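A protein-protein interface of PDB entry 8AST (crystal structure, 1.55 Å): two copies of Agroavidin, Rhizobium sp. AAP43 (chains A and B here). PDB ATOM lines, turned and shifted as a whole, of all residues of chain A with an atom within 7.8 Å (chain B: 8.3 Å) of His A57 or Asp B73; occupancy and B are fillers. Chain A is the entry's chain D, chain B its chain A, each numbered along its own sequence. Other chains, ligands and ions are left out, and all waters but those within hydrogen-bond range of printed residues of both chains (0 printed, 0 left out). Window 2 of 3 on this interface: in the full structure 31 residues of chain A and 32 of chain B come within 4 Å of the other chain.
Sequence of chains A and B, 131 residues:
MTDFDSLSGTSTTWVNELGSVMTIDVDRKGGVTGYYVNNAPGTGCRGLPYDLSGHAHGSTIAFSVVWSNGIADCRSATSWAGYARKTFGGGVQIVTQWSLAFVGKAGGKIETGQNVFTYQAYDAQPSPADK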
ATOM      1  N   ASP A   3     -20.735 -34.633  -4.505  1.00  0.00           N
ATOM      2  CA  ASP A   3     -20.808 -33.853  -5.762  1.00  0.00           C
ATOM      3  C   ASP A   3     -21.800 -32.699  -5.581  1.00  0.00           C
ATOM      4  O   ASP A   3     -22.875 -32.934  -4.993  1.00  0.00           O
ATOM      5  CB  ASP A   3     -21.293 -34.754  -6.896  1.00  0.00           C
ATOM      6  CG  ASP A   3     -20.936 -34.256  -8.271  1.00  0.00           C
ATOM      7  OD1 ASP A   3     -19.745 -34.035  -8.507  1.00  0.00           O
ATOM      8  OD2 ASP A   3     -21.847 -34.127  -9.091  1.00  0.00           O
ATOM      9  N   PHE A   4     -21.518 -31.510  -6.109  1.00  0.00           N
ATOM     10  CA  PHE A   4     -22.468 -30.372  -5.994  1.00  0.00           C
ATOM     11  C   PHE A   4     -23.705 -30.640  -6.842  1.00  0.00           C
ATOM     12  O   PHE A   4     -24.762 -30.139  -6.473  1.00  0.00           O
ATOM     13  CB  PHE A   4     -21.824 -29.018  -6.303  1.00  0.00           C
ATOM     14  CG  PHE A   4     -20.859 -28.611  -5.220  1.00  0.00           C
ATOM     15  CD1 PHE A   4     -21.333 -28.336  -3.941  1.00  0.00           C
ATOM     16  CD2 PHE A   4     -19.489 -28.542  -5.450  1.00  0.00           C
ATOM     17  CE1 PHE A   4     -20.454 -28.001  -2.920  1.00  0.00           C
ATOM     18  CE2 PHE A   4     -18.614 -28.240  -4.428  1.00  0.00           C
ATOM     19  CZ  PHE A   4     -19.095 -27.973  -3.163  1.00  0.00           C
ATOM     20  N   ASP A   5     -23.602 -31.431  -7.912  1.00  0.00           N
ATOM     21  CA  ASP A   5     -24.807 -31.760  -8.722  1.00  0.00           C
ATOM     22  C   ASP A   5     -25.782 -32.565  -7.835  1.00  0.00           C
ATOM     23  O   ASP A   5     -26.997 -32.379  -8.010  1.00  0.00           O
ATOM     24  CB  ASP A   5     -24.440 -32.398 -10.072  1.00  0.00           C
ATOM     25  CG  ASP A   5     -23.271 -31.725 -10.790  1.00  0.00           C
ATOM     26  OD1 ASP A   5     -23.237 -30.464 -10.858  1.00  0.00           O
ATOM     27  OD2 ASP A   5     -22.382 -32.467 -11.248  1.00  0.00           O
ATOM     28  N   VAL A  26     -29.317 -25.054  -4.019  1.00  0.00           N
ATOM     29  CA  VAL A  26     -28.661 -25.302  -5.322  1.00  0.00           C
ATOM     30  C   VAL A  26     -29.778 -25.757  -6.254  1.00  0.00           C
ATOM     31  O   VAL A  26     -30.503 -26.696  -5.912  1.00  0.00           O
ATOM     32  CB  VAL A  26     -27.564 -26.359  -5.184  1.00  0.00           C
ATOM     33  CG1 VAL A  26     -26.917 -26.626  -6.521  1.00  0.00           C
ATOM     34  CG2 VAL A  26     -26.527 -25.957  -4.133  1.00  0.00           C
ATOM     35  N   LYS A  29     -29.679 -26.350 -12.313  1.00  0.00           N
ATOM     36  CA  LYS A  29     -28.621 -25.868 -13.256  1.00  0.00           C
ATOM     37  C   LYS A  29     -27.343 -25.476 -12.489  1.00  0.00           C
ATOM     38  O   LYS A  29     -26.416 -24.930 -13.136  1.00  0.00           O
ATOM     39  CB  LYS A  29     -29.012 -24.591 -14.012  1.00  0.00           C
ATOM     40  CG  LYS A  29     -30.365 -24.578 -14.693  1.00  0.00           C
ATOM     41  CD  LYS A  29     -30.809 -23.177 -15.096  1.00  0.00           C
ATOM     42  CE  LYS A  29     -29.737 -22.349 -15.787  1.00  0.00           C
ATOM     43  NZ  LYS A  29     -30.314 -21.237 -16.589  1.00  0.00           N
ATOM     44  N   GLY A  30     -27.327 -25.655 -11.171  1.00  0.00           N
ATOM     45  CA  GLY A  30     -26.166 -25.318 -10.324  1.00  0.00           C
ATOM     46  C   GLY A  30     -26.201 -23.887  -9.770  1.00  0.00           C
ATOM     47  O   GLY A  30     -25.176 -23.477  -9.142  1.00  0.00           O
ATOM     48  N   GLY A  31     -27.280 -23.129  -9.990  1.00  0.00           N
ATOM     49  CA  GLY A  31     -27.419 -21.785  -9.404  1.00  0.00           C
ATOM     50  C   GLY A  31     -27.479 -21.902  -7.890  1.00  0.00           C
ATOM     51  O   GLY A  31     -28.166 -22.813  -7.360  1.00  0.00           O
ATOM     52  N   VAL A  32     -26.766 -21.025  -7.180  1.00  0.00           N
ATOM     53  CA  VAL A  32     -26.684 -21.059  -5.699  1.00  0.00           C
ATOM     54  C   VAL A  32     -27.273 -19.763  -5.188  1.00  0.00           C
ATOM     55  O   VAL A  32     -26.838 -18.671  -5.658  1.00  0.00           O
ATOM     56  CB  VAL A  32     -25.245 -21.212  -5.196  1.00  0.00           C
ATOM     57  CG1 VAL A  32     -25.206 -21.195  -3.670  1.00  0.00           C
ATOM     58  CG2 VAL A  32     -24.587 -22.461  -5.727  1.00  0.00           C
ATOM     59  N   HIS A  55     -22.623 -20.181  -7.826  1.00  0.00           N
ATOM     60  CA  HIS A  55     -22.806 -21.292  -8.781  1.00  0.00           C
ATOM     61  C   HIS A  55     -21.976 -22.472  -8.324  1.00  0.00           C
ATOM     62  O   HIS A  55     -20.880 -22.288  -7.816  1.00  0.00           O
ATOM     63  CB  HIS A  55     -22.395 -20.873 -10.192  1.00  0.00           C
ATOM     64  CG  HIS A  55     -23.173 -21.612 -11.210  1.00  0.00           C
ATOM     65  ND1 HIS A  55     -22.740 -22.830 -11.754  1.00  0.00           N
ATOM     66  CD2 HIS A  55     -24.424 -21.410 -11.674  1.00  0.00           C
ATOM     67  CE1 HIS A  55     -23.692 -23.293 -12.544  1.00  0.00           C
ATOM     68  NE2 HIS A  55     -24.706 -22.423 -12.532  1.00  0.00           N
ATOM     69  N   ALA A  56     -22.453 -23.670  -8.631  1.00  0.00           N
ATOM     70  CA  ALA A  56     -21.702 -24.905  -8.358  1.00  0.00           C
ATOM     71  C   ALA A  56     -21.810 -25.785  -9.580  1.00  0.00           C
ATOM     72  O   ALA A  56     -22.878 -25.828 -10.164  1.00  0.00           O
ATOM     73  CB  ALA A  56     -22.266 -25.566  -7.143  1.00  0.00           C
ATOM     74  N   HIS A  57     -20.743 -26.504  -9.882  1.00  0.00           N
ATOM     75  CA  HIS A  57     -20.773 -27.525 -10.952  1.00  0.00           C
ATOM     76  C   HIS A  57     -19.732 -28.592 -10.614  1.00  0.00           C
ATOM     77  O   HIS A  57     -18.574 -28.245 -10.300  1.00  0.00           O
ATOM     78  CB  HIS A  57     -20.525 -26.843 -12.299  1.00  0.00           C
ATOM     79  CG  HIS A  57     -20.454 -27.824 -13.405  1.00  0.00           C
ATOM     80  ND1 HIS A  57     -21.592 -28.322 -14.016  1.00  0.00           N
ATOM     81  CD2 HIS A  57     -19.399 -28.413 -14.002  1.00  0.00           C
ATOM     82  CE1 HIS A  57     -21.219 -29.153 -14.979  1.00  0.00           C
ATOM     83  NE2 HIS A  57     -19.895 -29.222 -14.982  1.00  0.00           N
ATOM     84  N   GLY A  58     -20.125 -29.862 -10.681  1.00  0.00           N
ATOM     85  CA  GLY A  58     -19.171 -30.953 -10.419  1.00  0.00           C
ATOM     86  C   GLY A  58     -18.654 -30.837  -9.004  1.00  0.00           C
ATOM     87  O   GLY A  58     -19.513 -30.768  -8.104  1.00  0.00           O
ATOM     88  N   SER A  59     -17.332 -30.760  -8.855  1.00  0.00           N
ATOM     89  CA  SER A  59     -16.648 -30.725  -7.537  1.00  0.00           C
ATOM     90  C   SER A  59     -16.278 -29.304  -7.129  1.00  0.00           C
ATOM     91  O   SER A  59     -15.554 -29.191  -6.133  1.00  0.00           O
ATOM     92  CB  SER A  59     -15.447 -31.593  -7.522  1.00  0.00           C
ATOM     93  OG  SER A  59     -15.888 -32.935  -7.656  1.00  0.00           O
ATOM     94  N   THR A  60     -16.697 -28.258  -7.844  1.00  0.00           N
ATOM     95  CA  THR A  60     -16.276 -26.892  -7.439  1.00  0.00           C
ATOM     96  C   THR A  60     -17.497 -25.982  -7.284  1.00  0.00           C
ATOM     97  O   THR A  60     -18.573 -26.245  -7.792  1.00  0.00           O
ATOM     98  CB  THR A  60     -15.169 -26.260  -8.296  1.00  0.00           C
ATOM     99  OG1 THR A  60     -15.775 -25.893  -9.537  1.00  0.00           O
ATOM    100  CG2 THR A  60     -13.944 -27.136  -8.449  1.00  0.00           C
ATOM    101  N   ILE A  61     -17.307 -24.932  -6.498  1.00  0.00           N
ATOM    102  CA  ILE A  61     -18.383 -23.993  -6.108  1.00  0.00           C
ATOM    103  C   ILE A  61     -17.733 -22.627  -5.919  1.00  0.00           C
ATOM    104  O   ILE A  61     -16.546 -22.524  -5.551  1.00  0.00           O
ATOM    105  CB  ILE A  61     -19.121 -24.467  -4.843  1.00  0.00           C
ATOM    106  CG1 ILE A  61     -20.351 -23.611  -4.547  1.00  0.00           C
ATOM    107  CG2 ILE A  61     -18.164 -24.495  -3.645  1.00  0.00           C
ATOM    108  CD1 ILE A  61     -21.340 -24.241  -3.585  1.00  0.00           C
ATOM    109  N   ALA A  62     -18.505 -21.577  -6.183  1.00  0.00           N
ATOM    110  CA  ALA A  62     -18.050 -20.216  -5.837  1.00  0.00           C
ATOM    111  C   ALA A  62     -19.267 -19.406  -5.437  1.00  0.00           C
ATOM    112  O   ALA A  62     -20.365 -19.659  -5.983  1.00  0.00           O
ATOM    113  CB  ALA A  62     -17.298 -19.617  -6.973  1.00  0.00           C
ATOM    114  N   GLY A  82     -14.272 -22.919  -3.857  1.00  0.00           N
ATOM    115  CA  GLY A  82     -13.988 -24.162  -3.128  1.00  0.00           C
ATOM    116  C   GLY A  82     -14.213 -25.407  -3.909  1.00  0.00           C
ATOM    117  O   GLY A  82     -14.792 -25.372  -5.026  1.00  0.00           O
ATOM    118  N   GLY B  44      -6.882 -23.343 -20.141  1.00  0.00           N
ATOM    119  CA  GLY B  44      -8.111 -23.924 -20.709  1.00  0.00           C
ATOM    120  C   GLY B  44      -9.265 -22.918 -20.640  1.00  0.00           C
ATOM    121  O   GLY B  44      -9.115 -21.917 -19.952  1.00  0.00           O
ATOM    122  N   CYS B  45     -10.386 -23.209 -21.281  1.00  0.00           N
ATOM    123  CA  CYS B  45     -11.642 -22.422 -21.183  1.00  0.00           C
ATOM    124  C   CYS B  45     -11.366 -20.982 -21.635  1.00  0.00           C
ATOM    125  O   CYS B  45     -11.726 -20.005 -20.952  1.00  0.00           O
ATOM    126  CB  CYS B  45     -12.196 -22.502 -19.774  1.00  0.00           C
ATOM    127  SG  CYS B  45     -12.769 -24.165 -19.349  1.00  0.00           S
ATOM    128  N   LEU B  48     -14.129 -18.011 -24.661  1.00  0.00           N
ATOM    129  CA  LEU B  48     -15.568 -18.337 -24.641  1.00  0.00           C
ATOM    130  C   LEU B  48     -16.174 -17.591 -23.473  1.00  0.00           C
ATOM    131  O   LEU B  48     -15.634 -17.641 -22.367  1.00  0.00           O
ATOM    132  CB  LEU B  48     -15.803 -19.838 -24.411  1.00  0.00           C
ATOM    133  CG  LEU B  48     -15.308 -20.819 -25.459  1.00  0.00           C
ATOM    134  CD1 LEU B  48     -15.400 -22.227 -24.878  1.00  0.00           C
ATOM    135  CD2 LEU B  48     -16.136 -20.701 -26.723  1.00  0.00           C
ATOM    136  N   TYR B  50     -18.108 -17.140 -20.135  1.00  0.00           N
ATOM    137  CA  TYR B  50     -18.671 -17.845 -18.956  1.00  0.00           C
ATOM    138  C   TYR B  50     -19.537 -16.857 -18.186  1.00  0.00           C
ATOM    139  O   TYR B  50     -19.249 -15.693 -18.066  1.00  0.00           O
ATOM    140  CB  TYR B  50     -17.553 -18.406 -18.081  1.00  0.00           C
ATOM    141  CG  TYR B  50     -16.819 -19.539 -18.729  1.00  0.00           C
ATOM    142  CD1 TYR B  50     -15.924 -19.328 -19.773  1.00  0.00           C
ATOM    143  CD2 TYR B  50     -17.156 -20.847 -18.422  1.00  0.00           C
ATOM    144  CE1 TYR B  50     -15.314 -20.397 -20.419  1.00  0.00           C
ATOM    145  CE2 TYR B  50     -16.572 -21.911 -19.072  1.00  0.00           C
ATOM    146  CZ  TYR B  50     -15.676 -21.693 -20.106  1.00  0.00           C
ATOM    147  OH  TYR B  50     -15.163 -22.742 -20.816  1.00  0.00           O
ATOM    148  N   VAL B  66     -17.894 -20.025 -12.471  1.00  0.00           N
ATOM    149  CA  VAL B  66     -17.628 -21.483 -12.474  1.00  0.00           C
ATOM    150  C   VAL B  66     -17.291 -21.824 -13.920  1.00  0.00           C
ATOM    151  O   VAL B  66     -17.999 -21.334 -14.786  1.00  0.00           O
ATOM    152  CB  VAL B  66     -18.814 -22.284 -11.903  1.00  0.00           C
ATOM    153  CG1 VAL B  66     -18.598 -23.774 -12.037  1.00  0.00           C
ATOM    154  CG2 VAL B  66     -18.950 -21.957 -10.434  1.00  0.00           C
ATOM    155  N   TRP B  67     -16.157 -22.468 -14.164  1.00  0.00           N
ATOM    156  CA  TRP B  67     -15.614 -22.632 -15.527  1.00  0.00           C
ATOM    157  C   TRP B  67     -16.262 -23.830 -16.225  1.00  0.00           C
ATOM    158  O   TRP B  67     -15.562 -24.785 -16.563  1.00  0.00           O
ATOM    159  CB  TRP B  67     -14.128 -22.748 -15.441  1.00  0.00           C
ATOM    160  CG  TRP B  67     -13.536 -21.477 -14.921  1.00  0.00           C
ATOM    161  CD1 TRP B  67     -13.087 -21.245 -13.654  1.00  0.00           C
ATOM    162  CD2 TRP B  67     -13.324 -20.258 -15.658  1.00  0.00           C
ATOM    163  NE1 TRP B  67     -12.628 -19.956 -13.540  1.00  0.00           N
ATOM    164  CE2 TRP B  67     -12.766 -19.328 -14.751  1.00  0.00           C
ATOM    165  CE3 TRP B  67     -13.574 -19.845 -16.977  1.00  0.00           C
ATOM    166  CZ2 TRP B  67     -12.426 -18.038 -15.143  1.00  0.00           C
ATOM    167  CZ3 TRP B  67     -13.233 -18.568 -17.350  1.00  0.00           C
ATOM    168  CH2 TRP B  67     -12.714 -17.661 -16.428  1.00  0.00           C
ATOM    169  N   SER B  68     -17.563 -23.758 -16.361  1.00  0.00           N
ATOM    170  CA  SER B  68     -18.383 -24.721 -17.147  1.00  0.00           C
ATOM    171  C   SER B  68     -19.500 -23.927 -17.797  1.00  0.00           C
ATOM    172  O   SER B  68     -20.281 -23.280 -17.075  1.00  0.00           O
ATOM    173  CB  SER B  68     -18.919 -25.823 -16.268  1.00  0.00           C
ATOM    174  OG  SER B  68     -19.799 -26.683 -17.013  1.00  0.00           O
ATOM    175  N   ASN B  69     -19.614 -23.954 -19.113  1.00  0.00           N
ATOM    176  CA  ASN B  69     -20.627 -23.141 -19.814  1.00  0.00           C
ATOM    177  C   ASN B  69     -21.396 -24.012 -20.815  1.00  0.00           C
ATOM    178  O   ASN B  69     -22.049 -23.445 -21.679  1.00  0.00           O
ATOM    179  CB  ASN B  69     -20.004 -21.937 -20.520  1.00  0.00           C
ATOM    180  CG  ASN B  69     -18.923 -22.325 -21.504  1.00  0.00           C
ATOM    181  OD1 ASN B  69     -18.626 -23.536 -21.674  1.00  0.00           O
ATOM    182  ND2 ASN B  69     -18.291 -21.337 -22.124  1.00  0.00           N
ATOM    183  N   GLY B  70     -21.249 -25.325 -20.702  1.00  0.00           N
ATOM    184  CA  GLY B  70     -21.890 -26.273 -21.629  1.00  0.00           C
ATOM    185  C   GLY B  70     -21.129 -26.459 -22.923  1.00  0.00           C
ATOM    186  O   GLY B  70     -21.551 -27.309 -23.728  1.00  0.00           O
ATOM    187  N   ILE B  71     -19.986 -25.785 -23.084  1.00  0.00           N
ATOM    188  CA  ILE B  71     -19.044 -25.931 -24.225  1.00  0.00           C
ATOM    189  C   ILE B  71     -17.708 -26.481 -23.736  1.00  0.00           C
ATOM    190  O   ILE B  71     -17.222 -27.462 -24.329  1.00  0.00           O
ATOM    191  CB  ILE B  71     -18.864 -24.589 -24.922  1.00  0.00           C
ATOM    192  CG1 ILE B  71     -20.194 -24.049 -25.454  1.00  0.00           C
ATOM    193  CG2 ILE B  71     -17.790 -24.679 -26.006  1.00  0.00           C
ATOM    194  CD1 ILE B  71     -20.106 -22.623 -26.028  1.00  0.00           C
ATOM    195  N   ALA B  72     -17.043 -25.822 -22.764  1.00  0.00           N
ATOM    196  CA  ALA B  72     -15.782 -26.336 -22.206  1.00  0.00           C
ATOM    197  C   ALA B  72     -15.871 -26.247 -20.681  1.00  0.00           C
ATOM    198  O   ALA B  72     -16.282 -25.213 -20.178  1.00  0.00           O
ATOM    199  CB  ALA B  72     -14.582 -25.611 -22.760  1.00  0.00           C
ATOM    200  N   ASP B  73     -15.413 -27.287 -20.012  1.00  0.00           N
ATOM    201  CA  ASP B  73     -15.410 -27.441 -18.545  1.00  0.00           C
ATOM    202  C   ASP B  73     -13.961 -27.552 -18.098  1.00  0.00           C
ATOM    203  O   ASP B  73     -13.253 -28.488 -18.518  1.00  0.00           O
ATOM    204  CB  ASP B  73     -16.296 -28.623 -18.134  1.00  0.00           C
ATOM    205  CG  ASP B  73     -16.353 -28.919 -16.637  1.00  0.00           C
ATOM    206  OD1 ASP B  73     -15.857 -28.115 -15.861  1.00  0.00           O
ATOM    207  OD2 ASP B  73     -16.888 -29.983 -16.264  1.00  0.00           O
ATOM    208  N   CYS B  74     -13.495 -26.643 -17.256  1.00  0.00           N
ATOM    209  CA  CYS B  74     -12.123 -26.701 -16.722  1.00  0.00           C
ATOM    210  C   CYS B  74     -12.142 -27.176 -15.256  1.00  0.00           C
ATOM    211  O   CYS B  74     -11.091 -27.040 -14.628  1.00  0.00           O
ATOM    212  CB  CYS B  74     -11.398 -25.379 -16.883  1.00  0.00           C
ATOM    213  SG  CYS B  74     -11.043 -25.035 -18.626  1.00  0.00           S
ATOM    214  N   ARG B  75     -13.266 -27.694 -14.770  1.00  0.00           N
ATOM    215  CA  ARG B  75     -13.354 -28.336 -13.428  1.00  0.00           C
ATOM    216  C   ARG B  75     -12.777 -27.364 -12.393  1.00  0.00           C
ATOM    217  O   ARG B  75     -11.936 -27.741 -11.523  1.00  0.00           O
ATOM    218  CB  ARG B  75     -12.654 -29.698 -13.451  1.00  0.00           C
ATOM    219  CG  ARG B  75     -13.314 -30.698 -14.399  1.00  0.00           C
ATOM    220  CD  ARG B  75     -12.584 -32.026 -14.272  1.00  0.00           C
ATOM    221  NE  ARG B  75     -12.943 -33.053 -15.248  1.00  0.00           N
ATOM    222  CZ  ARG B  75     -13.635 -34.172 -15.007  1.00  0.00           C
ATOM    223  NH1 ARG B  75     -13.867 -35.027 -15.996  1.00  0.00           N
ATOM    224  NH2 ARG B  75     -14.100 -34.437 -13.794  1.00  0.00           N
ATOM    225  N   SER B  76     -13.209 -26.120 -12.446  1.00  0.00           N
ATOM    226  CA  SER B  76     -12.659 -25.075 -11.577  1.00  0.00           C
ATOM    227  C   SER B  76     -13.691 -23.964 -11.365  1.00  0.00           C
ATOM    228  O   SER B  76     -14.682 -23.886 -12.110  1.00  0.00           O
ATOM    229  CB  SER B  76     -11.389 -24.528 -12.136  1.00  0.00           C
ATOM    230  OG  SER B  76     -11.573 -24.054 -13.433  1.00  0.00           O
ATOM    231  N   ALA B  77     -13.425 -23.132 -10.367  1.00  0.00           N
ATOM    232  CA  ALA B  77     -14.238 -21.965 -10.003  1.00  0.00           C
ATOM    233  C   ALA B  77     -13.314 -20.865  -9.514  1.00  0.00           C
ATOM    234  O   ALA B  77     -12.341 -21.122  -8.785  1.00  0.00           O
ATOM    235  CB  ALA B  77     -15.238 -22.319  -8.932  1.00  0.00           C
ATOM    236  N   VAL B 103      -9.906 -29.122  -9.543  1.00  0.00           N
ATOM    237  CA  VAL B 103      -9.901 -30.614  -9.463  1.00  0.00           C
ATOM    238  C   VAL B 103     -10.531 -31.052  -8.135  1.00  0.00           C
ATOM    239  O   VAL B 103     -11.663 -30.564  -7.875  1.00  0.00           O
ATOM    240  CB  VAL B 103      -8.497 -31.204  -9.722  1.00  0.00           C
ATOM    241  CG1 VAL B 103      -8.458 -32.702  -9.495  1.00  0.00           C
ATOM    242  CG2 VAL B 103      -8.030 -30.887 -11.132  1.00  0.00           C
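The side-chain hydroxyl of Thr A60 sits close to the backbone carbonyl oxygen of Ser B76. A ring nitrogen (NE2) of His A57 sits at hydrogen-bond distance from the side-chain hydroxyl of Ser B68 (3.3 Å). OD2 of Asp B73 sits at hydrogen-bond distance from NE2 of His A57 (3.4 Å).
O of Arg B75 lies within hydrogen-bond range of N of Val B103 (3.2 Å). The backbone NH of Gly A82 lies within hydrogen-bond range of the backbone carbonyl oxygen of Ile A61, at 2.9 Å. The side-chain sulfur (SG) of Cys B45 forms a disulfide with the side-chain sulfur (SG) of Cys B74 (2.1 Å). The backbone carbonyl oxygen (O) of Cys B74 sits at hydrogen-bond distance from the side-chain hydroxyl (OG) of Ser B76 (3.3 Å). The backbone carbonyl oxygen of Ser B76 is in hydrogen-bond range of the backbone NH of Trp B67. The backbone carbonyl oxygen (O) of Lys A29 lies within hydrogen-bond range of a ring nitrogen (NE2) of His A55 (3.1 Å).
His A55 touches Val B66 (O to CG2, 3.3 Å). CB of His A57 touches CG1 of Val B66, 3.6 Å away. Val B103 touches Ser A59 (O to CB, 3.9 Å). CG2 of Thr A60 touches O of Arg B75, at 3.7 Å. Thr A60 touches Ala B77 (OG1 to CB, 3.7 Å). Ile A61 touches Ala B77. CB of Ala B77 touches CB of Ala A62, at 3.9 Å.
His A57 touches three residues of chain B. Asp B73 touches one residue of chain A. No residue of chain B comes within 4 Å of Ala A56. No residue of chain B comes within 4 Å of Gly A58. Of the printed residues of chain A, Ser B76 touches Thr A60 (3.4 Å). Printed residues of chain A within 4 Å of Ser B68: His A57 (3.3 Å). Of the printed residues of chain A, Arg B75 touches Thr A60. Printed residues of chain A within 4 Å of Val B103: Ser A59 (3.9 Å). Trp B67 touches none of the printed residues of chain A. The nearest residue of chain B that does not touch His A57 is Trp B67 (5.9 Å).
Hydrophobic or aromatic side chains of chain A that line the printed part of chain B: His A55, His A57 and Ala A62. Hydrophobic or aromatic side chains of chain B within 4 Å of the printed part of chain A: Val B66 and Ala B77. Along chain B the printed residues that touch a printed residue of chain A span positions 66 to 103. Among the printed residues, no Asp or Glu carboxylate lies within 4 Å of a Lys or Arg side-chain nitrogen of the other chain.
No position is printed for both chains. Of the 10 pairs that touch across the chains among the printed residues, none has its exchanged pair printed and touching as well.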
